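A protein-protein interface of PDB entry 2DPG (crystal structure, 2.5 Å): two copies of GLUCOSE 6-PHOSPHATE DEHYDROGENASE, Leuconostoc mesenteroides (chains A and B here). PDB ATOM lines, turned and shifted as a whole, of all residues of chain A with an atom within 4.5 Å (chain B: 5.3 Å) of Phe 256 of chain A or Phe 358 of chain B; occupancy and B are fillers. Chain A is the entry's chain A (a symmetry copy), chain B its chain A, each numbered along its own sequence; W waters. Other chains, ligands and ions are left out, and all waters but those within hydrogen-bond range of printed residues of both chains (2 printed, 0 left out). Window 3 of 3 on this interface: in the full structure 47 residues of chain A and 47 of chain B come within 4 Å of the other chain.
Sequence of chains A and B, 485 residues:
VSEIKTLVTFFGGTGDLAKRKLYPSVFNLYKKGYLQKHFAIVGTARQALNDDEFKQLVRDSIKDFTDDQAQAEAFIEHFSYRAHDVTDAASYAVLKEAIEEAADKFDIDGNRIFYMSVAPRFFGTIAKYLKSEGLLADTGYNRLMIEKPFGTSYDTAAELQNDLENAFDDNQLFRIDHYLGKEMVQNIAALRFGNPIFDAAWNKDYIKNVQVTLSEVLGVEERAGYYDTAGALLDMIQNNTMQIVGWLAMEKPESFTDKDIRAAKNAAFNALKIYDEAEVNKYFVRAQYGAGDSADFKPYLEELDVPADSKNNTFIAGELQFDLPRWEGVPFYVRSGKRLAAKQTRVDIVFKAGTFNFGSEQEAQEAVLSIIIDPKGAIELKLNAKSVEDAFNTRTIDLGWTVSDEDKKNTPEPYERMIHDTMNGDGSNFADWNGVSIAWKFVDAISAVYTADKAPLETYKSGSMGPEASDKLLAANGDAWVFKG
The backbone NH of Phe 358 of chain B sits at hydrogen-bond distance from the side-chain carboxylate of Glu 363 of chain B, at 3.0 Å.
Among the printed residues, pairs that only touch across the chains: Phe 193 of chain A with Phe 356 of chain B, Phe 193 of chain A with Phe 358 of chain B, Gly 194 of chain A with Phe 358 of chain B, Gly 194 of chain A with Ala 364 of chain B, Phe 256 of chain A with Phe 356 of chain B, Phe 256 of chain A with Asn 357 of chain B, Phe 256 of chain A with Phe 358 of chain B and Phe 256 of chain A with Phe 392 of chain B.
Of the printed residues of chain B, Phe 256 of chain A touches Phe 356 (3.8 Å), Asn 357 (3.9 Å), Phe 358 (3.6 Å) and Phe 392 (3.7 Å).
Of chain A, only Phe 193 (3.9 Å), Gly 194 (3.6 Å) and Phe 256 (3.6 Å) come within 4 Å of Phe 358 of chain B.
Printed residues of chain B within 4 Å of Gly 194 of chain A: Phe 358 and Ala 364.
Of the printed residues of chain A, Phe 392 of chain B touches Phe 256 (3.7 Å).
Of the printed residues of chain A, Asn 357 of chain B touches Phe 256.
Printed residues of chain B within 4 Å of Phe 193 of chain A: Phe 356 and Phe 358.
The nearest printed residue of chain B that does not touch Phe 256 of chain A is Gly 359 of chain B (5.3 Å).
The nearest residue of chain A that does not touch Phe 358 of chain B is Ala 189 of chain A (4.1 Å).
Of the 9 printed residues of chain B, 5 touch a printed residue of chain A.
Hydrophobic or aromatic side chains of chain B within 4 Å of the printed part of chain A: Phe 356, Phe 358, Ala 364 and Phe 392.
Of the 9 printed residues of chain A, 3 touch a printed residue of chain B.
Hydrophobic or aromatic side chains of chain A within 4 Å of the printed part of chain B: Phe 193 and Phe 256.
No position is printed for both chains.
Of the 8 pairs that touch across the chains among the printed residues, none has its exchanged pair printed and touching as well.
Water W2 bridges the backbone carbonyl oxygen of Phe 193 of chain A and the backbone NH of Phe 356 of chain B.
Water W1 bridges N of Phe 256 of chain A (2.8 Å) and O of Asn 357 of chain B (3.2 Å).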
ATOM      1  N   ALA A 189       5.094  -7.323 -14.804  1.00  0.00           N
ATOM      2  CA  ALA A 189       3.813  -6.806 -15.275  1.00  0.00           C
ATOM      3  C   ALA A 189       3.991  -5.429 -15.914  1.00  0.00           C
ATOM      4  O   ALA A 189       3.349  -5.117 -16.912  1.00  0.00           O
ATOM      5  CB  ALA A 189       2.809  -6.740 -14.132  1.00  0.00           C
ATOM      6  N   ALA A 190       4.903  -4.632 -15.368  1.00  0.00           N
ATOM      7  CA  ALA A 190       5.164  -3.292 -15.879  1.00  0.00           C
ATOM      8  C   ALA A 190       5.768  -3.326 -17.281  1.00  0.00           C
ATOM      9  O   ALA A 190       5.292  -2.637 -18.180  1.00  0.00           O
ATOM     10  CB  ALA A 190       6.085  -2.540 -14.926  1.00  0.00           C
ATOM     11  N   PHE A 193       2.735  -5.180 -19.693  1.00  0.00           N
ATOM     12  CA  PHE A 193       1.551  -4.334 -19.874  1.00  0.00           C
ATOM     13  C   PHE A 193       1.810  -2.850 -20.096  1.00  0.00           C
ATOM     14  O   PHE A 193       0.996  -2.164 -20.710  1.00  0.00           O
ATOM     15  CB  PHE A 193       0.600  -4.506 -18.696  1.00  0.00           C
ATOM     16  CG  PHE A 193       0.224  -5.933 -18.433  1.00  0.00           C
ATOM     17  CD1 PHE A 193      -0.291  -6.733 -19.450  1.00  0.00           C
ATOM     18  CD2 PHE A 193       0.366  -6.472 -17.159  1.00  0.00           C
ATOM     19  CE1 PHE A 193      -0.661  -8.047 -19.194  1.00  0.00           C
ATOM     20  CE2 PHE A 193       0.000  -7.779 -16.898  1.00  0.00           C
ATOM     21  CZ  PHE A 193      -0.516  -8.572 -17.917  1.00  0.00           C
ATOM     22  N   GLY A 194       2.928  -2.350 -19.578  1.00  0.00           N
ATOM     23  CA  GLY A 194       3.259  -0.946 -19.736  1.00  0.00           C
ATOM     24  C   GLY A 194       3.865  -0.606 -21.085  1.00  0.00           C
ATOM     25  O   GLY A 194       3.983   0.571 -21.431  1.00  0.00           O
ATOM     26  N   SER A 255      -8.147  -5.216 -14.959  1.00  0.00           N
ATOM     27  CA  SER A 255      -7.556  -4.036 -14.352  1.00  0.00           C
ATOM     28  C   SER A 255      -6.389  -4.557 -13.527  1.00  0.00           C
ATOM     29  O   SER A 255      -6.182  -5.766 -13.460  1.00  0.00           O
ATOM     30  CB  SER A 255      -8.572  -3.302 -13.466  1.00  0.00           C
ATOM     31  OG  SER A 255      -8.898  -4.046 -12.307  1.00  0.00           O
ATOM     32  N   PHE A 256      -5.642  -3.667 -12.890  1.00  0.00           N
ATOM     33  CA  PHE A 256      -4.504  -4.085 -12.094  1.00  0.00           C
ATOM     34  C   PHE A 256      -4.830  -4.212 -10.607  1.00  0.00           C
ATOM     35  O   PHE A 256      -4.020  -3.853  -9.751  1.00  0.00           O
ATOM     36  CB  PHE A 256      -3.335  -3.128 -12.313  1.00  0.00           C
ATOM     37  CG  PHE A 256      -1.994  -3.759 -12.101  1.00  0.00           C
ATOM     38  CD1 PHE A 256      -1.621  -4.880 -12.830  1.00  0.00           C
ATOM     39  CD2 PHE A 256      -1.097  -3.230 -11.179  1.00  0.00           C
ATOM     40  CE1 PHE A 256      -0.369  -5.463 -12.647  1.00  0.00           C
ATOM     41  CE2 PHE A 256       0.161  -3.808 -10.987  1.00  0.00           C
ATOM     42  CZ  PHE A 256       0.525  -4.928 -11.726  1.00  0.00           C
ATOM     43  N   THR A 257      -6.021  -4.712 -10.302  1.00  0.00           N
ATOM     44  CA  THR A 257      -6.437  -4.908  -8.919  1.00  0.00           C
ATOM     45  C   THR A 257      -6.143  -6.356  -8.553  1.00  0.00           C
ATOM     46  O   THR A 257      -6.236  -7.233  -9.414  1.00  0.00           O
ATOM     47  CB  THR A 257      -7.929  -4.647  -8.757  1.00  0.00           C
ATOM     48  OG1 THR A 257      -8.653  -5.499  -9.649  1.00  0.00           O
ATOM     49  CG2 THR A 257      -8.237  -3.203  -9.088  1.00  0.00           C
ATOM     50  N   ASP A 258      -5.840  -6.620  -7.283  1.00  0.00           N
ATOM     51  CA  ASP A 258      -5.516  -7.974  -6.848  1.00  0.00           C
ATOM     52  C   ASP A 258      -6.479  -9.065  -7.317  1.00  0.00           C
ATOM     53  O   ASP A 258      -6.042 -10.131  -7.737  1.00  0.00           O
ATOM     54  CB  ASP A 258      -5.269  -8.046  -5.332  1.00  0.00           C
ATOM     55  CG  ASP A 258      -6.438  -7.535  -4.507  1.00  0.00           C
ATOM     56  OD1 ASP A 258      -7.463  -7.102  -5.077  1.00  0.00           O
ATOM     57  OD2 ASP A 258      -6.316  -7.560  -3.264  1.00  0.00           O
ATOM     58  N   ILE A 261      -5.874  -9.671 -11.086  1.00  0.00           N
ATOM     59  CA  ILE A 261      -4.540 -10.226 -11.270  1.00  0.00           C
ATOM     60  C   ILE A 261      -4.566 -11.706 -10.917  1.00  0.00           C
ATOM     61  O   ILE A 261      -4.006 -12.532 -11.644  1.00  0.00           O
ATOM     62  CB  ILE A 261      -3.512  -9.500 -10.394  1.00  0.00           C
ATOM     63  CG1 ILE A 261      -3.332  -8.069 -10.904  1.00  0.00           C
ATOM     64  CG2 ILE A 261      -2.186 -10.285 -10.347  1.00  0.00           C
ATOM     65  CD1 ILE A 261      -2.437  -7.234 -10.041  1.00  0.00           C
ATOM     66  N   PHE B 356      -3.182   0.506 -20.805  1.00  0.00           N
ATOM     67  CA  PHE B 356      -3.493  -0.341 -19.662  1.00  0.00           C
ATOM     68  C   PHE B 356      -3.360   0.530 -18.423  1.00  0.00           C
ATOM     69  O   PHE B 356      -2.341   1.178 -18.224  1.00  0.00           O
ATOM     70  CB  PHE B 356      -2.516  -1.517 -19.594  1.00  0.00           C
ATOM     71  CG  PHE B 356      -2.819  -2.505 -18.500  1.00  0.00           C
ATOM     72  CD1 PHE B 356      -3.751  -3.516 -18.697  1.00  0.00           C
ATOM     73  CD2 PHE B 356      -2.161  -2.433 -17.279  1.00  0.00           C
ATOM     74  CE1 PHE B 356      -4.021  -4.442 -17.689  1.00  0.00           C
ATOM     75  CE2 PHE B 356      -2.427  -3.353 -16.269  1.00  0.00           C
ATOM     76  CZ  PHE B 356      -3.356  -4.358 -16.473  1.00  0.00           C
ATOM     77  N   ASN B 357      -4.393   0.576 -17.597  1.00  0.00           N
ATOM     78  CA  ASN B 357      -4.332   1.398 -16.402  1.00  0.00           C
ATOM     79  C   ASN B 357      -3.878   0.619 -15.199  1.00  0.00           C
ATOM     80  O   ASN B 357      -4.515  -0.352 -14.789  1.00  0.00           O
ATOM     81  CB  ASN B 357      -5.688   2.032 -16.109  1.00  0.00           C
ATOM     82  CG  ASN B 357      -6.141   2.963 -17.208  1.00  0.00           C
ATOM     83  OD1 ASN B 357      -5.480   3.961 -17.501  1.00  0.00           O
ATOM     84  ND2 ASN B 357      -7.275   2.640 -17.831  1.00  0.00           N
ATOM     85  N   PHE B 358      -2.771   1.059 -14.624  1.00  0.00           N
ATOM     86  CA  PHE B 358      -2.230   0.429 -13.430  1.00  0.00           C
ATOM     87  C   PHE B 358      -2.924   0.976 -12.180  1.00  0.00           C
ATOM     88  O   PHE B 358      -3.043   0.284 -11.180  1.00  0.00           O
ATOM     89  CB  PHE B 358      -0.720   0.662 -13.347  1.00  0.00           C
ATOM     90  CG  PHE B 358       0.059  -0.023 -14.439  1.00  0.00           C
ATOM     91  CD1 PHE B 358       0.366  -1.378 -14.343  1.00  0.00           C
ATOM     92  CD2 PHE B 358       0.472   0.679 -15.572  1.00  0.00           C
ATOM     93  CE1 PHE B 358       1.075  -2.023 -15.355  1.00  0.00           C
ATOM     94  CE2 PHE B 358       1.182   0.043 -16.590  1.00  0.00           C
ATOM     95  CZ  PHE B 358       1.484  -1.315 -16.478  1.00  0.00           C
ATOM     96  N   GLY B 359      -3.448   2.195 -12.276  1.00  0.00           N
ATOM     97  CA  GLY B 359      -4.103   2.816 -11.140  1.00  0.00           C
ATOM     98  C   GLY B 359      -3.067   3.511 -10.276  1.00  0.00           C
ATOM     99  O   GLY B 359      -3.274   3.742  -9.083  1.00  0.00           O
ATOM    100  N   SER B 360      -1.942   3.844 -10.898  1.00  0.00           N
ATOM    101  CA  SER B 360      -0.834   4.515 -10.236  1.00  0.00           C
ATOM    102  C   SER B 360      -0.817   6.005 -10.557  1.00  0.00           C
ATOM    103  O   SER B 360      -1.560   6.464 -11.421  1.00  0.00           O
ATOM    104  CB  SER B 360       0.474   3.879 -10.703  1.00  0.00           C
ATOM    105  OG  SER B 360       0.461   3.696 -12.112  1.00  0.00           O
ATOM    106  N   GLU B 363       1.113   6.841 -15.069  1.00  0.00           N
ATOM    107  CA  GLU B 363       0.679   5.771 -15.947  1.00  0.00           C
ATOM    108  C   GLU B 363       1.741   5.573 -17.020  1.00  0.00           C
ATOM    109  O   GLU B 363       2.705   6.343 -17.106  1.00  0.00           O
ATOM    110  CB  GLU B 363      -0.680   6.082 -16.573  1.00  0.00           C
ATOM    111  CG  GLU B 363      -1.853   6.040 -15.582  1.00  0.00           C
ATOM    112  CD  GLU B 363      -2.164   4.645 -15.030  1.00  0.00           C
ATOM    113  OE1 GLU B 363      -1.655   3.637 -15.566  1.00  0.00           O
ATOM    114  OE2 GLU B 363      -2.945   4.560 -14.059  1.00  0.00           O
ATOM    115  N   ALA B 364       1.606   4.480 -17.764  1.00  0.00           N
ATOM    116  CA  ALA B 364       2.536   4.142 -18.832  1.00  0.00           C
ATOM    117  C   ALA B 364       2.783   5.325 -19.748  1.00  0.00           C
ATOM    118  O   ALA B 364       1.847   5.999 -20.166  1.00  0.00           O
ATOM    119  CB  ALA B 364       2.005   2.968 -19.631  1.00  0.00           C
ATOM    120  N   PHE B 392       2.875   0.763  -5.957  1.00  0.00           N
ATOM    121  CA  PHE B 392       3.161   0.425  -7.343  1.00  0.00           C
ATOM    122  C   PHE B 392       3.030   1.663  -8.221  1.00  0.00           C
ATOM    123  O   PHE B 392       2.012   2.360  -8.177  1.00  0.00           O
ATOM    124  CB  PHE B 392       2.217  -0.660  -7.855  1.00  0.00           C
ATOM    125  CG  PHE B 392       2.618  -1.218  -9.190  1.00  0.00           C
ATOM    126  CD1 PHE B 392       2.207  -0.607 -10.374  1.00  0.00           C
ATOM    127  CD2 PHE B 392       3.438  -2.332  -9.266  1.00  0.00           C
ATOM    128  CE1 PHE B 392       2.611  -1.098 -11.611  1.00  0.00           C
ATOM    129  CE2 PHE B 392       3.848  -2.834 -10.501  1.00  0.00           C
ATOM    130  CZ  PHE B 392       3.435  -2.216 -11.672  1.00  0.00           C
ATOM    131  N   THR B 394       4.828   3.472 -12.177  1.00  0.00           N
ATOM    132  CA  THR B 394       5.689   3.257 -13.331  1.00  0.00           C
ATOM    133  C   THR B 394       6.742   4.362 -13.422  1.00  0.00           C
ATOM    134  O   THR B 394       6.651   5.395 -12.748  1.00  0.00           O
ATOM    135  CB  THR B 394       4.896   3.187 -14.667  1.00  0.00           C
ATOM    136  OG1 THR B 394       4.348   4.473 -14.976  1.00  0.00           O
ATOM    137  CG2 THR B 394       3.775   2.164 -14.580  1.00  0.00           C
HETATM  138  O   HOH W   1      -6.222  -0.996 -12.215  1.00  0.00           O
HETATM  139  O   HOH W   2       0.081   0.459 -20.613  1.00  0.00           O
